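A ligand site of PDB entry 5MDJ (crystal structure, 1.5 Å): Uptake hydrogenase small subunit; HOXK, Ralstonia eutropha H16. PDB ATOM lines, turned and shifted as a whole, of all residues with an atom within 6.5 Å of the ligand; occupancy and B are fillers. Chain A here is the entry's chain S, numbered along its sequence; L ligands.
N of Arg 192 sits close to SG of Cys 190, 3.5 Å away. The backbone carbonyl oxygen of Ile 243 sits at hydrogen-bond distance from the guanidinium group of Arg 192 (3.0 Å). The backbone NH (N) of Cys 249 sits close to the side-chain sulfur (SG) of Cys 221 (3.5 Å). The side-chain sulfur (SG) of Cys 215 sits close to the backbone NH (N) of Tyr 217. O of Phe 214 lies within hydrogen-bond range of NH1 of Arg 192. N of Gly 223 lies close to SG of Cys 221 (3.4 Å). O of His 187 is in hydrogen-bond range of NH1 of Arg 193 (3.0 Å). The backbone carbonyl oxygen (O) of Leu 216 sits at hydrogen-bond distance from the backbone NH (N) of Cys 221, at 3.2 Å.
Merely in contact with the ligand: Ile 243 (3.7 Å), Arg 192 (3.7 Å), Gly 223 (3.8 Å), Tyr 217 (3.8 Å), Phe 196 (3.9 Å) and Pro 224 (3.9 Å). Hydrophobic or aromatic side chains that line the ligand: His 187, Phe 196, Leu 216, Tyr 217, Pro 224 and Ile 243. 12 residues have an atom within 4 Å of the ligand: His 187, Cys 190, Arg 192, Arg 193, Phe 196, Cys 215, Leu 216, Tyr 217, Cys 221, Gly 223, Pro 224 and Ile 243. The nearest printed residue that does not touch the ligand is Ile 186 (4.1 Å).
An iron atom (FE2) of the ligand is bound by the side-chain sulfur of Cys 215 (2.3 Å). The backbone NH (N) of Arg 193 lies close to a sulfur (S1) of the ligand (3.6 Å). The backbone NH (N) of Leu 216 lies close to a sulfur (S4) of the ligand (3.4 Å). The side-chain sulfur (SG) of Cys 221 binds an iron atom (FE1) of the ligand (2.3 Å). The side-chain sulfur (SG) of Cys 190 is bound to an iron atom (FE3) of the ligand (2.3 Å). An iron atom (FE4) of the ligand is bound by a ring nitrogen (ND1) of His 187 (2.1 Å).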
ATOM      1  N   ILE A 186     -10.842  12.196 -30.033  1.00  0.00           N
ATOM      2  CA  ILE A 186      -9.998  12.985 -30.940  1.00  0.00           C
ATOM      3  C   ILE A 186      -8.602  13.176 -30.330  1.00  0.00           C
ATOM      4  O   ILE A 186      -7.578  13.076 -30.985  1.00  0.00           O
ATOM      5  CB  ILE A 186     -10.598  14.391 -31.202  1.00  0.00           C
ATOM      6  CG1 ILE A 186     -12.043  14.385 -31.721  1.00  0.00           C
ATOM      7  CG2 ILE A 186      -9.783  15.172 -32.194  1.00  0.00           C
ATOM      8  CD1 ILE A 186     -12.259  13.569 -32.914  1.00  0.00           C
ATOM      9  N   HIS A 187      -8.588  13.468 -29.038  1.00  0.00           N
ATOM     10  CA  HIS A 187      -7.362  13.785 -28.304  1.00  0.00           C
ATOM     11  C   HIS A 187      -6.346  12.633 -28.227  1.00  0.00           C
ATOM     12  O   HIS A 187      -5.141  12.890 -28.061  1.00  0.00           O
ATOM     13  CB  HIS A 187      -7.803  14.337 -26.942  1.00  0.00           C
ATOM     14  CG  HIS A 187      -6.705  14.766 -26.036  1.00  0.00           C
ATOM     15  ND1 HIS A 187      -6.130  16.020 -26.101  1.00  0.00           N
ATOM     16  CD2 HIS A 187      -6.147  14.157 -24.964  1.00  0.00           C
ATOM     17  CE1 HIS A 187      -5.229  16.135 -25.139  1.00  0.00           C
ATOM     18  NE2 HIS A 187      -5.228  15.022 -24.435  1.00  0.00           N
ATOM     19  N   ASP A 188      -6.810  11.388 -28.358  1.00  0.00           N
ATOM     20  CA  ASP A 188      -5.935  10.208 -28.241  1.00  0.00           C
ATOM     21  C   ASP A 188      -4.784  10.267 -29.243  1.00  0.00           C
ATOM     22  O   ASP A 188      -3.623  10.137 -28.876  1.00  0.00           O
ATOM     23  CB  ASP A 188      -6.729   8.891 -28.441  1.00  0.00           C
ATOM     24  CG  ASP A 188      -7.785   8.604 -27.320  1.00  0.00           C
ATOM     25  OD1 ASP A 188      -7.746   9.254 -26.262  1.00  0.00           O
ATOM     26  OD2 ASP A 188      -8.638   7.683 -27.505  1.00  0.00           O
ATOM     27  N   CYS A 190      -4.617  12.898 -31.815  1.00  0.00           N
ATOM     28  CA  CYS A 190      -4.426  14.236 -32.383  1.00  0.00           C
ATOM     29  C   CYS A 190      -2.940  14.558 -32.560  1.00  0.00           C
ATOM     30  O   CYS A 190      -2.168  14.433 -31.624  1.00  0.00           O
ATOM     31  CB  CYS A 190      -5.050  15.275 -31.480  1.00  0.00           C
ATOM     32  SG  CYS A 190      -4.876  16.975 -32.065  1.00  0.00           S
ATOM     33  N   TYR A 191      -2.561  15.005 -33.744  1.00  0.00           N
ATOM     34  CA  TYR A 191      -1.142  15.323 -34.022  1.00  0.00           C
ATOM     35  C   TYR A 191      -0.574  16.470 -33.156  1.00  0.00           C
ATOM     36  O   TYR A 191       0.640  16.616 -33.048  1.00  0.00           O
ATOM     37  CB  TYR A 191      -0.903  15.571 -35.537  1.00  0.00           C
ATOM     38  CG  TYR A 191      -1.248  16.965 -35.953  1.00  0.00           C
ATOM     39  CD1 TYR A 191      -2.575  17.391 -35.995  1.00  0.00           C
ATOM     40  CD2 TYR A 191      -0.240  17.901 -36.241  1.00  0.00           C
ATOM     41  CE1 TYR A 191      -2.879  18.702 -36.323  1.00  0.00           C
ATOM     42  CE2 TYR A 191      -0.536  19.211 -36.558  1.00  0.00           C
ATOM     43  CZ  TYR A 191      -1.867  19.597 -36.600  1.00  0.00           C
ATOM     44  OH  TYR A 191      -2.188  20.879 -36.899  1.00  0.00           O
ATOM     45  N   ARG A 192      -1.446  17.259 -32.509  1.00  0.00           N
ATOM     46  CA  ARG A 192      -0.991  18.336 -31.607  1.00  0.00           C
ATOM     47  C   ARG A 192      -0.779  17.848 -30.193  1.00  0.00           C
ATOM     48  O   ARG A 192      -0.405  18.640 -29.320  1.00  0.00           O
ATOM     49  CB  ARG A 192      -1.950  19.543 -31.626  1.00  0.00           C
ATOM     50  CG  ARG A 192      -2.146  20.160 -33.000  1.00  0.00           C
ATOM     51  CD  ARG A 192      -2.733  21.556 -32.956  1.00  0.00           C
ATOM     52  NE  ARG A 192      -2.899  22.090 -34.313  1.00  0.00           N
ATOM     53  CZ  ARG A 192      -2.961  23.379 -34.645  1.00  0.00           C
ATOM     54  NH1 ARG A 192      -2.863  24.346 -33.724  1.00  0.00           N
ATOM     55  NH2 ARG A 192      -3.103  23.730 -35.925  1.00  0.00           N
ATOM     56  N   ARG A 193      -0.988  16.552 -29.953  1.00  0.00           N
ATOM     57  CA  ARG A 193      -0.844  15.979 -28.608  1.00  0.00           C
ATOM     58  C   ARG A 193       0.517  16.204 -27.943  1.00  0.00           C
ATOM     59  O   ARG A 193       0.557  16.504 -26.759  1.00  0.00           O
ATOM     60  CB  ARG A 193      -1.246  14.488 -28.616  1.00  0.00           C
ATOM     61  CG  ARG A 193      -1.314  13.804 -27.271  1.00  0.00           C
ATOM     62  CD  ARG A 193      -2.316  14.425 -26.327  1.00  0.00           C
ATOM     63  NE  ARG A 193      -2.222  13.726 -25.059  1.00  0.00           N
ATOM     64  CZ  ARG A 193      -2.792  12.562 -24.773  1.00  0.00           C
ATOM     65  NH1 ARG A 193      -3.544  11.933 -25.665  1.00  0.00           N
ATOM     66  NH2 ARG A 193      -2.603  12.005 -23.584  1.00  0.00           N
ATOM     67  N   PRO A 194       1.618  16.107 -28.708  1.00  0.00           N
ATOM     68  CA  PRO A 194       2.915  16.387 -28.064  1.00  0.00           C
ATOM     69  C   PRO A 194       3.015  17.815 -27.504  1.00  0.00           C
ATOM     70  O   PRO A 194       3.637  18.024 -26.453  1.00  0.00           O
ATOM     71  CB  PRO A 194       3.918  16.158 -29.195  1.00  0.00           C
ATOM     72  CG  PRO A 194       3.262  15.089 -30.035  1.00  0.00           C
ATOM     73  CD  PRO A 194       1.806  15.496 -30.036  1.00  0.00           C
ATOM     74  N   HIS A 195       2.388  18.772 -28.177  1.00  0.00           N
ATOM     75  CA  HIS A 195       2.314  20.124 -27.652  1.00  0.00           C
ATOM     76  C   HIS A 195       1.476  20.179 -26.372  1.00  0.00           C
ATOM     77  O   HIS A 195       1.906  20.755 -25.387  1.00  0.00           O
ATOM     78  CB  HIS A 195       1.773  21.112 -28.688  1.00  0.00           C
ATOM     79  CG  HIS A 195       2.689  21.342 -29.849  1.00  0.00           C
ATOM     80  ND1 HIS A 195       3.967  21.834 -29.696  1.00  0.00           N
ATOM     81  CD2 HIS A 195       2.518  21.164 -31.176  1.00  0.00           C
ATOM     82  CE1 HIS A 195       4.541  21.953 -30.886  1.00  0.00           C
ATOM     83  NE2 HIS A 195       3.679  21.544 -31.797  1.00  0.00           N
ATOM     84  N   PHE A 196       0.316  19.547 -26.374  1.00  0.00           N
ATOM     85  CA  PHE A 196      -0.504  19.449 -25.161  1.00  0.00           C
ATOM     86  C   PHE A 196       0.304  18.859 -23.990  1.00  0.00           C
ATOM     87  O   PHE A 196       0.273  19.376 -22.880  1.00  0.00           O
ATOM     88  CB  PHE A 196      -1.730  18.571 -25.411  1.00  0.00           C
ATOM     89  CG  PHE A 196      -2.582  18.356 -24.190  1.00  0.00           C
ATOM     90  CD1 PHE A 196      -2.327  17.302 -23.318  1.00  0.00           C
ATOM     91  CD2 PHE A 196      -3.638  19.201 -23.905  1.00  0.00           C
ATOM     92  CE1 PHE A 196      -3.121  17.112 -22.200  1.00  0.00           C
ATOM     93  CE2 PHE A 196      -4.420  19.030 -22.786  1.00  0.00           C
ATOM     94  CZ  PHE A 196      -4.164  17.965 -21.923  1.00  0.00           C
ATOM     95  N   PHE A 201       0.552  25.811 -25.764  1.00  0.00           N
ATOM     96  CA  PHE A 201      -0.812  26.179 -26.134  1.00  0.00           C
ATOM     97  C   PHE A 201      -0.890  27.510 -26.873  1.00  0.00           C
ATOM     98  O   PHE A 201      -0.162  28.441 -26.587  1.00  0.00           O
ATOM     99  CB  PHE A 201      -1.679  26.297 -24.890  1.00  0.00           C
ATOM    100  CG  PHE A 201      -1.748  25.049 -24.063  1.00  0.00           C
ATOM    101  CD1 PHE A 201      -2.501  23.950 -24.483  1.00  0.00           C
ATOM    102  CD2 PHE A 201      -1.063  24.972 -22.858  1.00  0.00           C
ATOM    103  CE1 PHE A 201      -2.553  22.801 -23.715  1.00  0.00           C
ATOM    104  CE2 PHE A 201      -1.126  23.835 -22.082  1.00  0.00           C
ATOM    105  CZ  PHE A 201      -1.866  22.754 -22.510  1.00  0.00           C
ATOM    106  N   PHE A 214       0.538  24.978 -32.084  1.00  0.00           N
ATOM    107  CA  PHE A 214       0.433  24.537 -30.697  1.00  0.00           C
ATOM    108  C   PHE A 214      -0.992  24.069 -30.397  1.00  0.00           C
ATOM    109  O   PHE A 214      -1.942  24.341 -31.150  1.00  0.00           O
ATOM    110  CB  PHE A 214       0.882  25.644 -29.737  1.00  0.00           C
ATOM    111  CG  PHE A 214       2.377  25.766 -29.556  1.00  0.00           C
ATOM    112  CD1 PHE A 214       3.277  25.105 -30.383  1.00  0.00           C
ATOM    113  CD2 PHE A 214       2.872  26.558 -28.543  1.00  0.00           C
ATOM    114  CE1 PHE A 214       4.646  25.217 -30.180  1.00  0.00           C
ATOM    115  CE2 PHE A 214       4.235  26.691 -28.352  1.00  0.00           C
ATOM    116  CZ  PHE A 214       5.121  26.011 -29.171  1.00  0.00           C
ATOM    117  N   CYS A 215      -1.141  23.311 -29.306  1.00  0.00           N
ATOM    118  CA  CYS A 215      -2.425  22.751 -28.913  1.00  0.00           C
ATOM    119  C   CYS A 215      -3.499  23.828 -28.715  1.00  0.00           C
ATOM    120  O   CYS A 215      -3.205  24.927 -28.212  1.00  0.00           O
ATOM    121  CB  CYS A 215      -2.239  21.934 -27.650  1.00  0.00           C
ATOM    122  SG  CYS A 215      -3.768  21.345 -26.868  1.00  0.00           S
ATOM    123  N   LEU A 216      -4.732  23.492 -29.076  1.00  0.00           N
ATOM    124  CA  LEU A 216      -5.866  24.384 -29.056  1.00  0.00           C
ATOM    125  C   LEU A 216      -6.767  24.243 -27.803  1.00  0.00           C
ATOM    126  O   LEU A 216      -7.830  24.867 -27.728  1.00  0.00           O
ATOM    127  CB  LEU A 216      -6.692  24.222 -30.340  1.00  0.00           C
ATOM    128  CG  LEU A 216      -5.902  24.553 -31.622  1.00  0.00           C
ATOM    129  CD1 LEU A 216      -6.653  24.064 -32.849  1.00  0.00           C
ATOM    130  CD2 LEU A 216      -5.637  26.045 -31.716  1.00  0.00           C
ATOM    131  N   TYR A 217      -6.322  23.494 -26.805  1.00  0.00           N
ATOM    132  CA  TYR A 217      -7.115  23.304 -25.556  1.00  0.00           C
ATOM    133  C   TYR A 217      -7.581  24.620 -24.937  1.00  0.00           C
ATOM    134  O   TYR A 217      -8.743  24.772 -24.546  1.00  0.00           O
ATOM    135  CB  TYR A 217      -6.292  22.532 -24.522  1.00  0.00           C
ATOM    136  CG  TYR A 217      -7.023  22.115 -23.270  1.00  0.00           C
ATOM    137  CD1 TYR A 217      -7.668  20.897 -23.196  1.00  0.00           C
ATOM    138  CD2 TYR A 217      -7.047  22.943 -22.163  1.00  0.00           C
ATOM    139  CE1 TYR A 217      -8.315  20.483 -22.033  1.00  0.00           C
ATOM    140  CE2 TYR A 217      -7.703  22.550 -21.001  1.00  0.00           C
ATOM    141  CZ  TYR A 217      -8.335  21.320 -20.946  1.00  0.00           C
ATOM    142  OH  TYR A 217      -8.990  20.907 -19.794  1.00  0.00           O
ATOM    143  N   LYS A 218      -6.650  25.563 -24.782  1.00  0.00           N
ATOM    144  CA  LYS A 218      -7.009  26.850 -24.156  1.00  0.00           C
ATOM    145  C   LYS A 218      -7.864  27.766 -25.025  1.00  0.00           C
ATOM    146  O   LYS A 218      -8.401  28.757 -24.533  1.00  0.00           O
ATOM    147  CB  LYS A 218      -5.728  27.553 -23.632  1.00  0.00           C
ATOM    148  CG  LYS A 218      -5.037  26.732 -22.556  1.00  0.00           C
ATOM    149  CD  LYS A 218      -3.832  27.462 -21.983  1.00  0.00           C
ATOM    150  CE  LYS A 218      -3.318  26.667 -20.792  1.00  0.00           C
ATOM    151  NZ  LYS A 218      -2.085  27.274 -20.213  1.00  0.00           N
ATOM    152  N   CYS A 221     -10.839  23.784 -27.443  1.00  0.00           N
ATOM    153  CA  CYS A 221     -10.903  22.483 -28.101  1.00  0.00           C
ATOM    154  C   CYS A 221     -11.574  21.419 -27.224  1.00  0.00           C
ATOM    155  O   CYS A 221     -11.173  21.185 -26.110  1.00  0.00           O
ATOM    156  CB  CYS A 221      -9.509  21.980 -28.482  1.00  0.00           C
ATOM    157  SG  CYS A 221      -9.565  20.458 -29.459  1.00  0.00           S
ATOM    158  N   LYS A 222     -12.581  20.752 -27.789  1.00  0.00           N
ATOM    159  CA  LYS A 222     -13.335  19.725 -27.078  1.00  0.00           C
ATOM    160  C   LYS A 222     -12.889  18.330 -27.476  1.00  0.00           C
ATOM    161  O   LYS A 222     -13.552  17.334 -27.146  1.00  0.00           O
ATOM    162  CB  LYS A 222     -14.841  19.945 -27.265  1.00  0.00           C
ATOM    163  CG  LYS A 222     -15.327  21.283 -26.710  1.00  0.00           C
ATOM    164  CD  LYS A 222     -14.757  21.598 -25.325  1.00  0.00           C
ATOM    165  CE  LYS A 222     -15.377  22.787 -24.636  1.00  0.00           C
ATOM    166  NZ  LYS A 222     -15.382  24.021 -25.444  1.00  0.00           N
ATOM    167  N   GLY A 223     -11.765  18.232 -28.187  1.00  0.00           N
ATOM    168  CA  GLY A 223     -11.168  16.945 -28.514  1.00  0.00           C
ATOM    169  C   GLY A 223     -11.007  15.959 -27.383  1.00  0.00           C
ATOM    170  O   GLY A 223     -11.251  14.775 -27.584  1.00  0.00           O
ATOM    171  N   PRO A 224     -10.628  16.440 -26.181  1.00  0.00           N
ATOM    172  CA  PRO A 224     -10.481  15.496 -25.073  1.00  0.00           C
ATOM    173  C   PRO A 224     -11.737  14.773 -24.623  1.00  0.00           C
ATOM    174  O   PRO A 224     -11.605  13.769 -23.921  1.00  0.00           O
ATOM    175  CB  PRO A 224      -9.916  16.373 -23.940  1.00  0.00           C
ATOM    176  CG  PRO A 224      -9.245  17.508 -24.645  1.00  0.00           C
ATOM    177  CD  PRO A 224     -10.108  17.781 -25.830  1.00  0.00           C
ATOM    178  N   PHE A 241      -8.502  18.167 -40.814  1.00  0.00           N
ATOM    179  CA  PHE A 241      -9.612  18.105 -39.877  1.00  0.00           C
ATOM    180  C   PHE A 241      -9.622  19.432 -39.119  1.00  0.00           C
ATOM    181  O   PHE A 241      -8.672  20.212 -39.252  1.00  0.00           O
ATOM    182  CB  PHE A 241      -9.570  16.848 -38.992  1.00  0.00           C
ATOM    183  CG  PHE A 241      -8.505  16.838 -37.913  1.00  0.00           C
ATOM    184  CD1 PHE A 241      -7.166  16.751 -38.228  1.00  0.00           C
ATOM    185  CD2 PHE A 241      -8.873  16.731 -36.541  1.00  0.00           C
ATOM    186  CE1 PHE A 241      -6.191  16.608 -37.231  1.00  0.00           C
ATOM    187  CE2 PHE A 241      -7.908  16.569 -35.555  1.00  0.00           C
ATOM    188  CZ  PHE A 241      -6.559  16.552 -35.900  1.00  0.00           C
ATOM    189  N   ILE A 243      -8.892  20.689 -36.228  1.00  0.00           N
ATOM    190  CA  ILE A 243      -7.695  21.068 -35.468  1.00  0.00           C
ATOM    191  C   ILE A 243      -6.491  21.323 -36.374  1.00  0.00           C
ATOM    192  O   ILE A 243      -5.757  22.304 -36.168  1.00  0.00           O
ATOM    193  CB  ILE A 243      -7.401  20.010 -34.388  1.00  0.00           C
ATOM    194  CG1 ILE A 243      -8.451  20.114 -33.282  1.00  0.00           C
ATOM    195  CG2 ILE A 243      -5.995  20.090 -33.835  1.00  0.00           C
ATOM    196  CD1 ILE A 243      -8.792  18.789 -32.656  1.00  0.00           C
ATOM    197  N   GLY A 248     -10.309  24.652 -32.766  1.00  0.00           N
ATOM    198  CA  GLY A 248     -10.579  23.502 -31.900  1.00  0.00           C
ATOM    199  C   GLY A 248     -11.802  22.724 -32.313  1.00  0.00           C
ATOM    200  O   GLY A 248     -12.725  23.245 -32.964  1.00  0.00           O
ATOM    201  N   CYS A 249     -11.814  21.451 -31.952  1.00  0.00           N
ATOM    202  CA  CYS A 249     -13.015  20.642 -32.059  1.00  0.00           C
ATOM    203  C   CYS A 249     -14.102  21.340 -31.240  1.00  0.00           C
ATOM    204  O   CYS A 249     -13.821  21.829 -30.134  1.00  0.00           O
ATOM    205  CB  CYS A 249     -12.701  19.240 -31.506  1.00  0.00           C
ATOM    206  SG  CYS A 249     -14.101  18.117 -31.345  1.00  0.00           S
HETATM  207 FE1  LIG L   1      -7.487  19.496 -28.983  1.00  0.00          FE
HETATM  208 FE2  LIG L   1      -4.901  19.805 -28.117  1.00  0.00          FE
HETATM  209 FE3  LIG L   1      -5.475  18.074 -30.149  1.00  0.00          FE
HETATM  210 FE4  LIG L   1      -6.211  17.520 -27.601  1.00  0.00          FE
HETATM  211  S1  LIG L   1      -4.032  17.722 -28.411  1.00  0.00           S
HETATM  212  S2  LIG L   1      -7.525  17.230 -29.421  1.00  0.00           S
HETATM  213  S3  LIG L   1      -6.799  19.590 -26.819  1.00  0.00           S
HETATM  214  S4  LIG L   1      -5.692  20.362 -30.164  1.00  0.00           S
